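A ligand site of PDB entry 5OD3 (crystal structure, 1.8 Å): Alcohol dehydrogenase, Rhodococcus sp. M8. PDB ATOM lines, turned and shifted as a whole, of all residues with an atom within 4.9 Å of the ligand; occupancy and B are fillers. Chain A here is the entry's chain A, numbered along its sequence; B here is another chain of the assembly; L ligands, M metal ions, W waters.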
ATOM      1  N   CYS A  38      10.587   7.124 -18.914  1.00  0.00           N
ATOM      2  CA  CYS A  38       9.986   7.619 -20.137  1.00  0.00           C
ATOM      3  C   CYS A  38      10.995   8.462 -20.897  1.00  0.00           C
ATOM      4  O   CYS A  38      11.797   9.164 -20.294  1.00  0.00           O
ATOM      5  CB  CYS A  38       8.773   8.475 -19.786  1.00  0.00           C
ATOM      6  SG  CYS A  38       7.957   9.246 -21.203  1.00  0.00           S
ATOM      7  N   HIS A  39      10.911   8.443 -22.216  1.00  0.00           N
ATOM      8  CA  HIS A  39      11.855   9.229 -23.009  1.00  0.00           C
ATOM      9  C   HIS A  39      11.677  10.742 -22.766  1.00  0.00           C
ATOM     10  O   HIS A  39      12.610  11.516 -22.972  1.00  0.00           O
ATOM     11  CB  HIS A  39      11.764   8.893 -24.482  1.00  0.00           C
ATOM     12  CG  HIS A  39      13.038   9.139 -25.221  1.00  0.00           C
ATOM     13  ND1 HIS A  39      13.940   8.134 -25.490  1.00  0.00           N
ATOM     14  CD2 HIS A  39      13.581  10.279 -25.710  1.00  0.00           C
ATOM     15  CE1 HIS A  39      14.982   8.651 -26.136  1.00  0.00           C
ATOM     16  NE2 HIS A  39      14.781   9.945 -26.274  1.00  0.00           N
ATOM     17  N   SER A  40      10.502  11.160 -22.276  1.00  0.00           N
ATOM     18  CA  SER A  40      10.333  12.546 -21.842  1.00  0.00           C
ATOM     19  C   SER A  40      11.310  12.975 -20.733  1.00  0.00           C
ATOM     20  O   SER A  40      11.688  14.157 -20.651  1.00  0.00           O
ATOM     21  CB  SER A  40       8.896  12.823 -21.403  1.00  0.00           C
ATOM     22  OG  SER A  40       8.054  12.798 -22.544  1.00  0.00           O
ATOM     23  N   PHE A  43      14.354  13.978 -22.640  1.00  0.00           N
ATOM     24  CA  PHE A  43      14.103  15.303 -23.199  1.00  0.00           C
ATOM     25  C   PHE A  43      14.293  16.389 -22.159  1.00  0.00           C
ATOM     26  O   PHE A  43      15.005  17.352 -22.398  1.00  0.00           O
ATOM     27  CB  PHE A  43      12.710  15.420 -23.833  1.00  0.00           C
ATOM     28  CG  PHE A  43      12.495  16.745 -24.508  1.00  0.00           C
ATOM     29  CD1 PHE A  43      13.023  16.978 -25.773  1.00  0.00           C
ATOM     30  CD2 PHE A  43      11.843  17.784 -23.855  1.00  0.00           C
ATOM     31  CE1 PHE A  43      12.862  18.206 -26.378  1.00  0.00           C
ATOM     32  CE2 PHE A  43      11.684  19.013 -24.470  1.00  0.00           C
ATOM     33  CZ  PHE A  43      12.189  19.222 -25.733  1.00  0.00           C
ATOM     34  N   ASP A 153       1.245   6.737 -18.335  1.00  0.00           N
ATOM     35  CA  ASP A 153       1.769   7.632 -19.364  1.00  0.00           C
ATOM     36  C   ASP A 153       1.932   6.905 -20.683  1.00  0.00           C
ATOM     37  O   ASP A 153       1.345   7.310 -21.678  1.00  0.00           O
ATOM     38  CB  ASP A 153       3.060   8.204 -18.865  1.00  0.00           C
ATOM     39  CG  ASP A 153       3.589   9.336 -19.711  1.00  0.00           C
ATOM     40  OD1 ASP A 153       2.849  10.014 -20.461  1.00  0.00           O
ATOM     41  OD2 ASP A 153       4.795   9.542 -19.559  1.00  0.00           O
ATOM     42  N   THR A 157      -1.177   8.502 -22.457  1.00  0.00           N
ATOM     43  CA  THR A 157      -0.900   9.469 -23.531  1.00  0.00           C
ATOM     44  C   THR A 157      -1.389   8.982 -24.901  1.00  0.00           C
ATOM     45  O   THR A 157      -2.110   9.714 -25.576  1.00  0.00           O
ATOM     46  CB  THR A 157       0.550   9.902 -23.495  1.00  0.00           C
ATOM     47  OG1 THR A 157       0.792  10.566 -22.238  1.00  0.00           O
ATOM     48  CG2 THR A 157       0.872  10.861 -24.623  1.00  0.00           C
ATOM     49  N   ILE A 178       3.834   5.401 -35.541  1.00  0.00           N
ATOM     50  CA  ILE A 178       5.267   5.605 -35.772  1.00  0.00           C
ATOM     51  C   ILE A 178       6.005   5.603 -34.441  1.00  0.00           C
ATOM     52  O   ILE A 178       5.753   6.466 -33.599  1.00  0.00           O
ATOM     53  CB  ILE A 178       5.565   6.893 -36.522  1.00  0.00           C
ATOM     54  CG1 ILE A 178       4.708   7.000 -37.802  1.00  0.00           C
ATOM     55  CG2 ILE A 178       7.072   6.936 -36.866  1.00  0.00           C
ATOM     56  CD1 ILE A 178       4.928   8.281 -38.592  1.00  0.00           C
ATOM     57  N   GLY A 179       6.893   4.634 -34.273  1.00  0.00           N
ATOM     58  CA  GLY A 179       7.693   4.463 -33.037  1.00  0.00           C
ATOM     59  C   GLY A 179       7.067   3.426 -32.157  1.00  0.00           C
ATOM     60  O   GLY A 179       6.071   3.720 -31.500  1.00  0.00           O
ATOM     61  N   VAL A 180       7.645   2.225 -32.105  1.00  0.00           N
ATOM     62  CA  VAL A 180       7.105   1.100 -31.312  1.00  0.00           C
ATOM     63  C   VAL A 180       7.969   0.963 -30.036  1.00  0.00           C
ATOM     64  O   VAL A 180       8.666  -0.054 -29.815  1.00  0.00           O
ATOM     65  CB  VAL A 180       7.044  -0.172 -32.144  1.00  0.00           C
ATOM     66  CG1 VAL A 180       6.306  -1.299 -31.429  1.00  0.00           C
ATOM     67  CG2 VAL A 180       6.365   0.113 -33.470  1.00  0.00           C
ATOM     68  N   GLY A 181       7.946   2.020 -29.246  1.00  0.00           N
ATOM     69  CA  GLY A 181       8.644   2.100 -27.964  1.00  0.00           C
ATOM     70  C   GLY A 181       7.685   1.910 -26.823  1.00  0.00           C
ATOM     71  O   GLY A 181       6.710   1.191 -26.949  1.00  0.00           O
ATOM     72  N   GLY A 182       7.956   2.547 -25.687  1.00  0.00           N
ATOM     73  CA  GLY A 182       7.061   2.473 -24.576  1.00  0.00           C
ATOM     74  C   GLY A 182       5.628   2.855 -24.929  1.00  0.00           C
ATOM     75  O   GLY A 182       4.695   2.081 -24.722  1.00  0.00           O
ATOM     76  N   LEU A 183       5.467   4.058 -25.455  1.00  0.00           N
ATOM     77  CA  LEU A 183       4.139   4.554 -25.818  1.00  0.00           C
ATOM     78  C   LEU A 183       3.585   3.776 -27.009  1.00  0.00           C
ATOM     79  O   LEU A 183       2.446   3.304 -26.959  1.00  0.00           O
ATOM     80  CB  LEU A 183       4.167   6.048 -26.163  1.00  0.00           C
ATOM     81  CG  LEU A 183       3.912   7.002 -25.017  1.00  0.00           C
ATOM     82  CD1 LEU A 183       5.019   6.993 -23.987  1.00  0.00           C
ATOM     83  CD2 LEU A 183       3.726   8.431 -25.546  1.00  0.00           C
ATOM     84  N   GLY A 184       4.396   3.609 -28.042  1.00  0.00           N
ATOM     85  CA  GLY A 184       3.886   3.027 -29.296  1.00  0.00           C
ATOM     86  C   GLY A 184       3.399   1.600 -29.212  1.00  0.00           C
ATOM     87  O   GLY A 184       2.395   1.233 -29.851  1.00  0.00           O
ATOM     88  N   VAL A 202       5.474   1.413 -37.635  1.00  0.00           N
ATOM     89  CA  VAL A 202       6.666   1.955 -38.315  1.00  0.00           C
ATOM     90  C   VAL A 202       7.743   2.122 -37.265  1.00  0.00           C
ATOM     91  O   VAL A 202       7.516   2.730 -36.217  1.00  0.00           O
ATOM     92  CB  VAL A 202       6.376   3.297 -39.005  1.00  0.00           C
ATOM     93  CG1 VAL A 202       7.602   3.847 -39.729  1.00  0.00           C
ATOM     94  CG2 VAL A 202       5.203   3.178 -39.977  1.00  0.00           C
ATOM     95  N   ASP A 203       8.924   1.563 -37.495  1.00  0.00           N
ATOM     96  CA  ASP A 203      10.062   1.755 -36.572  1.00  0.00           C
ATOM     97  C   ASP A 203      11.381   1.595 -37.362  1.00  0.00           C
ATOM     98  O   ASP A 203      11.384   1.037 -38.454  1.00  0.00           O
ATOM     99  CB  ASP A 203       9.993   0.762 -35.402  1.00  0.00           C
ATOM    100  CG  ASP A 203      10.739   1.210 -34.187  1.00  0.00           C
ATOM    101  OD1 ASP A 203      12.004   1.249 -34.202  1.00  0.00           O
ATOM    102  OD2 ASP A 203      10.093   1.570 -33.180  1.00  0.00           O
ATOM    103  N   LEU A 204      12.445   2.145 -36.816  1.00  0.00           N
ATOM    104  CA  LEU A 204      13.801   1.999 -37.409  1.00  0.00           C
ATOM    105  C   LEU A 204      14.391   0.605 -37.177  1.00  0.00           C
ATOM    106  O   LEU A 204      15.200   0.157 -37.952  1.00  0.00           O
ATOM    107  CB  LEU A 204      14.765   3.017 -36.814  1.00  0.00           C
ATOM    108  CG  LEU A 204      14.537   4.487 -37.201  1.00  0.00           C
ATOM    109  CD1 LEU A 204      15.303   5.410 -36.261  1.00  0.00           C
ATOM    110  CD2 LEU A 204      14.876   4.737 -38.682  1.00  0.00           C
ATOM    111  N   ASP A 205      13.958  -0.048 -36.101  1.00  0.00           N
ATOM    112  CA  ASP A 205      14.570  -1.279 -35.579  1.00  0.00           C
ATOM    113  C   ASP A 205      13.657  -2.482 -35.911  1.00  0.00           C
ATOM    114  O   ASP A 205      12.494  -2.533 -35.521  1.00  0.00           O
ATOM    115  CB  ASP A 205      14.782  -1.083 -34.068  1.00  0.00           C
ATOM    116  CG  ASP A 205      15.448  -2.279 -33.363  1.00  0.00           C
ATOM    117  OD1 ASP A 205      15.443  -3.415 -33.892  1.00  0.00           O
ATOM    118  OD2 ASP A 205      15.966  -2.053 -32.245  1.00  0.00           O
ATOM    119  N   ARG A 208      11.828  -4.114 -33.127  1.00  0.00           N
ATOM    120  CA  ARG A 208      10.648  -3.367 -32.691  1.00  0.00           C
ATOM    121  C   ARG A 208       9.471  -3.579 -33.647  1.00  0.00           C
ATOM    122  O   ARG A 208       8.311  -3.573 -33.217  1.00  0.00           O
ATOM    123  CB  ARG A 208      10.947  -1.866 -32.527  1.00  0.00           C
ATOM    124  CG  ARG A 208      12.054  -1.580 -31.513  1.00  0.00           C
ATOM    125  CD  ARG A 208      11.792  -2.295 -30.200  1.00  0.00           C
ATOM    126  NE  ARG A 208      12.930  -2.136 -29.333  1.00  0.00           N
ATOM    127  CZ  ARG A 208      13.170  -1.035 -28.632  1.00  0.00           C
ATOM    128  NH1 ARG A 208      12.307  -0.013 -28.631  1.00  0.00           N
ATOM    129  NH2 ARG A 208      14.246  -0.974 -27.888  1.00  0.00           N
ATOM    130  N   SER A 223      10.966   2.407 -40.932  1.00  0.00           N
ATOM    131  CA  SER A 223      10.920   3.863 -40.978  1.00  0.00           C
ATOM    132  C   SER A 223      12.019   4.395 -41.869  1.00  0.00           C
ATOM    133  O   SER A 223      12.979   3.706 -42.149  1.00  0.00           O
ATOM    134  CB  SER A 223      11.078   4.466 -39.574  1.00  0.00           C
ATOM    135  OG  SER A 223      10.710   5.849 -39.591  1.00  0.00           O
ATOM    136  N   PHE A 246       4.684   8.814 -32.529  1.00  0.00           N
ATOM    137  CA  PHE A 246       5.301   8.757 -31.203  1.00  0.00           C
ATOM    138  C   PHE A 246       6.810   9.008 -31.233  1.00  0.00           C
ATOM    139  O   PHE A 246       7.486   8.821 -30.215  1.00  0.00           O
ATOM    140  CB  PHE A 246       4.992   7.420 -30.525  1.00  0.00           C
ATOM    141  CG  PHE A 246       3.527   7.176 -30.307  1.00  0.00           C
ATOM    142  CD1 PHE A 246       2.812   7.887 -29.345  1.00  0.00           C
ATOM    143  CD2 PHE A 246       2.840   6.292 -31.119  1.00  0.00           C
ATOM    144  CE1 PHE A 246       1.461   7.682 -29.147  1.00  0.00           C
ATOM    145  CE2 PHE A 246       1.474   6.080 -30.936  1.00  0.00           C
ATOM    146  CZ  PHE A 246       0.775   6.799 -29.959  1.00  0.00           C
ATOM    147  N   VAL A 247       7.328   9.437 -32.387  1.00  0.00           N
ATOM    148  CA  VAL A 247       8.723   9.879 -32.528  1.00  0.00           C
ATOM    149  C   VAL A 247       8.746  11.407 -32.579  1.00  0.00           C
ATOM    150  O   VAL A 247       9.391  12.051 -31.751  1.00  0.00           O
ATOM    151  CB  VAL A 247       9.357   9.281 -33.803  1.00  0.00           C
ATOM    152  CG1 VAL A 247      10.808   9.745 -34.011  1.00  0.00           C
ATOM    153  CG2 VAL A 247       9.324   7.759 -33.733  1.00  0.00           C
ATOM    154  N   SER A 251      11.526  14.141 -39.851  1.00  0.00           N
ATOM    155  CA  SER A 251      11.395  13.098 -40.851  1.00  0.00           C
ATOM    156  C   SER A 251      10.089  12.282 -40.695  1.00  0.00           C
ATOM    157  O   SER A 251       9.451  11.965 -41.689  1.00  0.00           O
ATOM    158  CB  SER A 251      12.596  12.133 -40.828  1.00  0.00           C
ATOM    159  OG  SER A 251      12.773  11.566 -39.557  1.00  0.00           O
ATOM    160  N   THR A 252       9.717  11.976 -39.468  1.00  0.00           N
ATOM    161  CA  THR A 252       8.490  11.200 -39.215  1.00  0.00           C
ATOM    162  C   THR A 252       7.224  12.032 -39.409  1.00  0.00           C
ATOM    163  O   THR A 252       6.242  11.538 -39.938  1.00  0.00           O
ATOM    164  CB  THR A 252       8.498  10.560 -37.807  1.00  0.00           C
ATOM    165  OG1 THR A 252       8.613  11.537 -36.791  1.00  0.00           O
ATOM    166  CG2 THR A 252       9.622   9.550 -37.684  1.00  0.00           C
ATOM    167  N   VAL A 269       2.784  13.251 -31.162  1.00  0.00           N
ATOM    168  CA  VAL A 269       2.904  12.945 -29.740  1.00  0.00           C
ATOM    169  C   VAL A 269       4.354  13.001 -29.284  1.00  0.00           C
ATOM    170  O   VAL A 269       4.636  13.544 -28.213  1.00  0.00           O
ATOM    171  CB  VAL A 269       2.318  11.547 -29.425  1.00  0.00           C
ATOM    172  CG1 VAL A 269       2.373  11.261 -27.942  1.00  0.00           C
ATOM    173  CG2 VAL A 269       0.889  11.458 -29.932  1.00  0.00           C
ATOM    174  N   GLY A 270       5.261  12.401 -30.071  1.00  0.00           N
ATOM    175  CA  GLY A 270       6.682  12.447 -29.769  1.00  0.00           C
ATOM    176  C   GLY A 270       7.256  13.841 -29.849  1.00  0.00           C
ATOM    177  O   GLY A 270       6.760  14.665 -30.614  1.00  0.00           O
ATOM    178  N   ILE A 271       8.280  14.112 -29.033  1.00  0.00           N
ATOM    179  CA  ILE A 271       8.866  15.450 -28.869  1.00  0.00           C
ATOM    180  C   ILE A 271      10.304  15.460 -29.389  1.00  0.00           C
ATOM    181  O   ILE A 271      11.146  14.741 -28.860  1.00  0.00           O
ATOM    182  CB  ILE A 271       8.859  15.914 -27.378  1.00  0.00           C
ATOM    183  CG1 ILE A 271       7.451  15.781 -26.778  1.00  0.00           C
ATOM    184  CG2 ILE A 271       9.284  17.383 -27.294  1.00  0.00           C
ATOM    185  CD1 ILE A 271       7.335  15.936 -25.276  1.00  0.00           C
ATOM    186  N   PRO A 293      -0.990  16.538 -28.752  1.00  0.00           N
ATOM    187  CA  PRO A 293      -1.736  16.291 -27.519  1.00  0.00           C
ATOM    188  C   PRO A 293      -0.792  16.222 -26.318  1.00  0.00           C
ATOM    189  O   PRO A 293       0.418  16.087 -26.497  1.00  0.00           O
ATOM    190  CB  PRO A 293      -2.382  14.946 -27.781  1.00  0.00           C
ATOM    191  CG  PRO A 293      -1.407  14.226 -28.622  1.00  0.00           C
ATOM    192  CD  PRO A 293      -0.739  15.285 -29.489  1.00  0.00           C
ATOM    193  N   TYR A 294      -1.340  16.402 -25.129  1.00  0.00           N
ATOM    194  CA  TYR A 294      -0.545  16.341 -23.877  1.00  0.00           C
ATOM    195  C   TYR A 294      -1.188  15.406 -22.892  1.00  0.00           C
ATOM    196  O   TYR A 294      -2.302  15.654 -22.456  1.00  0.00           O
ATOM    197  CB  TYR A 294      -0.408  17.719 -23.282  1.00  0.00           C
ATOM    198  CG  TYR A 294       0.281  17.746 -21.916  1.00  0.00           C
ATOM    199  CD1 TYR A 294       1.553  17.258 -21.730  1.00  0.00           C
ATOM    200  CD2 TYR A 294      -0.372  18.293 -20.830  1.00  0.00           C
ATOM    201  CE1 TYR A 294       2.180  17.334 -20.475  1.00  0.00           C
ATOM    202  CE2 TYR A 294       0.224  18.352 -19.564  1.00  0.00           C
ATOM    203  CZ  TYR A 294       1.501  17.867 -19.398  1.00  0.00           C
ATOM    204  OH  TYR A 294       2.063  17.919 -18.120  1.00  0.00           O
ATOM    205  N   TRP A 295      -0.465  14.333 -22.581  1.00  0.00           N
ATOM    206  CA  TRP A 295      -0.805  13.411 -21.493  1.00  0.00           C
ATOM    207  C   TRP A 295      -2.250  12.927 -21.650  1.00  0.00           C
ATOM    208  O   TRP A 295      -2.597  12.486 -22.762  1.00  0.00           O
ATOM    209  CB  TRP A 295      -0.446  14.032 -20.122  1.00  0.00           C
ATOM    210  CG  TRP A 295       0.122  13.049 -19.168  1.00  0.00           C
ATOM    211  CD1 TRP A 295      -0.129  11.716 -19.098  1.00  0.00           C
ATOM    212  CD2 TRP A 295       1.051  13.329 -18.103  1.00  0.00           C
ATOM    213  NE1 TRP A 295       0.593  11.133 -18.078  1.00  0.00           N
ATOM    214  CE2 TRP A 295       1.326  12.104 -17.450  1.00  0.00           C
ATOM    215  CE3 TRP A 295       1.685  14.491 -17.675  1.00  0.00           C
ATOM    216  CZ2 TRP A 295       2.197  12.022 -16.371  1.00  0.00           C
ATOM    217  CZ3 TRP A 295       2.547  14.415 -16.576  1.00  0.00           C
ATOM    218  CH2 TRP A 295       2.796  13.188 -15.950  1.00  0.00           C
ATOM    219  N   LEU A 332      17.874   3.479 -22.140  1.00  0.00           N
ATOM    220  CA  LEU A 332      16.780   4.147 -22.868  1.00  0.00           C
ATOM    221  C   LEU A 332      17.346   5.088 -23.922  1.00  0.00           C
ATOM    222  O   LEU A 332      16.895   5.059 -25.067  1.00  0.00           O
ATOM    223  CB  LEU A 332      15.839   4.895 -21.921  1.00  0.00           C
ATOM    224  CG  LEU A 332      14.557   5.458 -22.544  1.00  0.00           C
ATOM    225  CD1 LEU A 332      13.727   4.343 -23.175  1.00  0.00           C
ATOM    226  CD2 LEU A 332      13.743   6.227 -21.513  1.00  0.00           C
ATOM    227  N   GLY A 339      10.337  -2.189 -25.029  1.00  0.00           N
ATOM    228  CA  GLY A 339       9.112  -1.804 -24.359  1.00  0.00           C
ATOM    229  C   GLY A 339       9.442  -0.721 -23.349  1.00  0.00           C
ATOM    230  O   GLY A 339      10.139   0.259 -23.681  1.00  0.00           O
ATOM    231  N   ARG A 340       8.980  -0.905 -22.114  1.00  0.00           N
ATOM    232  CA  ARG A 340       9.141   0.096 -21.062  1.00  0.00           C
ATOM    233  C   ARG A 340      10.097  -0.373 -19.971  1.00  0.00           C
ATOM    234  O   ARG A 340       9.957  -1.488 -19.458  1.00  0.00           O
ATOM    235  CB  ARG A 340       7.787   0.366 -20.387  1.00  0.00           C
ATOM    236  CG  ARG A 340       7.205   1.710 -20.708  1.00  0.00           C
ATOM    237  CD  ARG A 340       7.940   2.805 -19.998  1.00  0.00           C
ATOM    238  NE  ARG A 340       7.240   4.090 -20.106  1.00  0.00           N
ATOM    239  CZ  ARG A 340       7.418   5.000 -21.066  1.00  0.00           C
ATOM    240  NH1 ARG A 340       8.254   4.801 -22.088  1.00  0.00           N
ATOM    241  NH2 ARG A 340       6.739   6.131 -20.976  1.00  0.00           N
ATOM    242  N   PHE B 281       5.640  21.079 -30.611  1.00  0.00           N
ATOM    243  CA  PHE B 281       5.774  21.441 -29.207  1.00  0.00           C
ATOM    244  C   PHE B 281       6.539  22.751 -29.038  1.00  0.00           C
ATOM    245  O   PHE B 281       7.462  23.023 -29.791  1.00  0.00           O
ATOM    246  CB  PHE B 281       6.434  20.297 -28.423  1.00  0.00           C
ATOM    247  CG  PHE B 281       5.545  19.105 -28.281  1.00  0.00           C
ATOM    248  CD1 PHE B 281       4.551  19.106 -27.316  1.00  0.00           C
ATOM    249  CD2 PHE B 281       5.626  18.036 -29.163  1.00  0.00           C
ATOM    250  CE1 PHE B 281       3.677  18.024 -27.184  1.00  0.00           C
ATOM    251  CE2 PHE B 281       4.762  16.972 -29.058  1.00  0.00           C
ATOM    252  CZ  PHE B 281       3.790  16.962 -28.068  1.00  0.00           C
HETATM  253  P1  LIG L   1      11.060   5.118 -26.396  1.00  0.00           P
HETATM  254  O1  LIG L   1      12.480   5.509 -26.270  1.00  0.00           O
HETATM  255  O2  LIG L   1      10.441   3.995 -25.580  1.00  0.00           O
HETATM  256  O3  LIG L   1      10.722   4.728 -27.892  1.00  0.00           O
HETATM  257  C1  LIG L   1      11.619   4.938 -28.941  1.00  0.00           C
HETATM  258  C2  LIG L   1      11.168   4.079 -30.100  1.00  0.00           C
HETATM  259  O4  LIG L   1      11.114   4.991 -31.186  1.00  0.00           O
HETATM  260  C3  LIG L   1      12.153   2.973 -30.459  1.00  0.00           C
HETATM  261  O5  LIG L   1      11.497   1.763 -30.847  1.00  0.00           O
HETATM  262  C4  LIG L   1      12.904   3.552 -31.639  1.00  0.00           C
HETATM  263  O6  LIG L   1      13.387   2.589 -32.558  1.00  0.00           O
HETATM  264  C5  LIG L   1      11.804   4.396 -32.270  1.00  0.00           C
HETATM  265  N1  LIG L   1      12.255   5.430 -33.190  1.00  0.00           N
HETATM  266  C6  LIG L   1      13.214   6.365 -32.962  1.00  0.00           C
HETATM  267  N2  LIG L   1      13.359   7.147 -34.053  1.00  0.00           N
HETATM  268  C7  LIG L   1      12.511   6.692 -35.002  1.00  0.00           C
HETATM  269  C8  LIG L   1      12.154   7.084 -36.341  1.00  0.00           C
HETATM  270  N3  LIG L   1      12.805   8.126 -36.935  1.00  0.00           N
HETATM  271  N4  LIG L   1      11.182   6.393 -36.982  1.00  0.00           N
HETATM  272  C9  LIG L   1      10.551   5.349 -36.374  1.00  0.00           C
HETATM  273  N5  LIG L   1      10.835   4.933 -35.138  1.00  0.00           N
HETATM  274  C10 LIG L   1      11.796   5.559 -34.427  1.00  0.00           C
HETATM  275  O7  LIG L   1      10.150   6.464 -26.273  1.00  0.00           O
HETATM  276  P2  LIG L   1       8.797   6.637 -25.395  1.00  0.00           P
HETATM  277  O8  LIG L   1       9.208   6.704 -23.921  1.00  0.00           O
HETATM  278  O9  LIG L   1       7.775   5.631 -25.898  1.00  0.00           O
HETATM  279  O10 LIG L   1       8.398   8.140 -25.785  1.00  0.00           O
HETATM  280  C11 LIG L   1       8.042   8.430 -27.139  1.00  0.00           C
HETATM  281  C12 LIG L   1       7.957   9.926 -27.354  1.00  0.00           C
HETATM  282  O11 LIG L   1       6.745  10.413 -26.789  1.00  0.00           O
HETATM  283  C13 LIG L   1       9.109  10.751 -26.766  1.00  0.00           C
HETATM  284  O12 LIG L   1       9.434  11.775 -27.717  1.00  0.00           O
HETATM  285  C14 LIG L   1       8.503  11.284 -25.506  1.00  0.00           C
HETATM  286  O13 LIG L   1       9.181  12.459 -25.055  1.00  0.00           O
HETATM  287  C15 LIG L   1       7.059  11.515 -25.946  1.00  0.00           C
HETATM  288  N6  LIG L   1       6.012  11.645 -24.922  1.00  0.00           N
HETATM  289  C16 LIG L   1       5.089  12.596 -25.132  1.00  0.00           C
HETATM  290  C17 LIG L   1       4.041  12.821 -24.269  1.00  0.00           C
HETATM  291  C18 LIG L   1       3.014  13.866 -24.573  1.00  0.00           C
HETATM  292  O14 LIG L   1       2.266  14.230 -23.661  1.00  0.00           O
HETATM  293  N7  LIG L   1       2.833  14.362 -25.824  1.00  0.00           N
HETATM  294  C19 LIG L   1       3.940  12.016 -23.130  1.00  0.00           C
HETATM  295  C20 LIG L   1       4.891  11.001 -22.933  1.00  0.00           C
HETATM  296  C21 LIG L   1       5.927  10.839 -23.831  1.00  0.00           C
HETATM  297 ZN    ZN M   1       6.420  10.472 -20.029  1.00  0.00          ZN
HETATM  298  O   HOH W   1      14.252   7.477 -29.897  1.00  0.00           O
HETATM  299  O   HOH W   2      14.601   9.637 -33.096  1.00  0.00           O
HETATM  300  O   HOH W   3      11.663  12.990 -25.971  1.00  0.00           O
HETATM  301  O   HOH W   4       6.996   4.826 -28.400  1.00  0.00           O
HETATM  302  O   HOH W   5      14.955   9.896 -36.149  1.00  0.00           O
HETATM  303  O   HOH W   6      11.505   1.474 -25.848  1.00  0.00           O
HETATM  304  O   HOH W   7      14.844   4.215 -26.507  1.00  0.00           O
HETATM  305  O   HOH W   8      10.303   3.016 -23.044  1.00  0.00           O
HETATM  306  O   HOH W   9      12.455   8.818 -39.865  1.00  0.00           O
HETATM  307  O   HOH W  10      10.835  10.958 -29.834  1.00  0.00           O
HETATM  308  O   HOH W  11       8.424   6.337 -30.216  1.00  0.00           O
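The side-chain carboxylate (OD1) of Asp 203 is in hydrogen-bond range of an oxygen (O6) of the ligand (2.5 Å).
The side-chain hydroxyl (OG) of Ser 223 sits at hydrogen-bond distance from a nitrogen (N4) of the ligand.
O13 of the ligand sits at hydrogen-bond distance from N of Ser 40, at 3.3 Å.
An oxygen (O13) of the ligand lies within hydrogen-bond range of the side-chain hydroxyl (OG) of Ser 40.
O8 of the ligand lies within salt-bridge range of NH1 of Arg 340 (2.8 Å).
The backbone NH (N) of Leu 183 is in hydrogen-bond range of an oxygen (O9) of the ligand.
The backbone NH (N) of Gly 182 is in hydrogen-bond range of an oxygen (O2) of the ligand (2.9 Å).
The backbone NH (N) of Ile 271 is in hydrogen-bond range of an oxygen (O12) of the ligand.
The backbone NH of Trp 295 sits at hydrogen-bond distance from an oxygen (O14) of the ligand (2.9 Å).
The guanidinium group of Arg 208 is in hydrogen-bond range of an oxygen (O5) of the ligand, at 3.0 Å.
N of His 39 sits at hydrogen-bond distance from O8 of the ligand (3.0 Å).
O1 of the ligand lies within hydrogen-bond range of ND1 of His 39.
N7 of the ligand sits at hydrogen-bond distance from O of Pro 293 (3.0 Å).
The backbone carbonyl oxygen of Val 269 is in hydrogen-bond range of a nitrogen (N7) of the ligand.
N of Ser 223 lies within hydrogen-bond range of O of Asp 203.
The side-chain carboxylate of Asp 203 lies within hydrogen-bond range of the backbone NH of Val 180 (2.8 Å).
The side-chain carboxylate of Asp 203 lies within hydrogen-bond range of the backbone NH of Asp 205, at 3.0 Å.
SG of Cys 38 lies close to N of Ser 40.
SG of Cys 38 lies close to NH2 of Arg 340.
The backbone NH (N) of Phe 246 lies within hydrogen-bond range of the backbone carbonyl oxygen (O) of Ile 178 (2.8 Å).
The side-chain hydroxyl of Thr 157 is in hydrogen-bond range of the side-chain carboxylate of Asp 153 (2.8 Å).
The backbone NH of Gly 179 lies within hydrogen-bond range of the backbone carbonyl oxygen of Val 202 (2.8 Å).
Cys 38 touches the ligand (SG to C21, 3.7 Å).
Asp 153 touches the ligand.
Thr 157 touches the ligand (OG1 to C19, 3.6 Å).
CG2 of Ile 178 touches C9 of the ligand (3.9 Å).
CA of Gly 179 touches N5 of the ligand (3.8 Å).
Val 180 touches the ligand (O to O5, 3.5 Å).
Gly 181 touches the ligand (CA to O3, 3.4 Å).
CD1 of Leu 204 touches C7 of the ligand, at 3.3 Å.
O of Phe 246 touches C12 of the ligand (3.1 Å).
Val 247 touches the ligand.
Thr 252 touches the ligand.
Gly 270 touches the ligand.
Tyr 294 touches the ligand (CA to O14, 3.5 Å).
CD1 of Leu 332 touches O1 of the ligand, at 3.5 Å.
Phe 281 of chain B touches the ligand (CZ to N7, 3.6 Å).
Of the 33 residues printed, 27 come within 4 Å of the ligand.
The nearest printed residue that does not touch the ligand is Val 202 (4.01 Å).
Water W10 bridges O of Val 247 (2.6 Å) and O12 of the ligand (2.7 Å).
Water W3 lies within hydrogen-bond range of O13 of the ligand (2.7 Å), O of Ile 271 (3.4 Å) and O of His 39 (3.5 Å).
Water W7 bridges O of Leu 332 (2.6 Å) and O1 of the ligand (2.7 Å).
Water W6 lies within hydrogen-bond range of O2 of the ligand, O of Gly 339 and NH1 of Arg 208.
Water W9 lies within hydrogen-bond range of OG of Ser 251, N3 of the ligand and OG of Ser 223.
Water W11 bridges O of Phe 246 (2.7 Å) and O4 of the ligand (3.2 Å).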
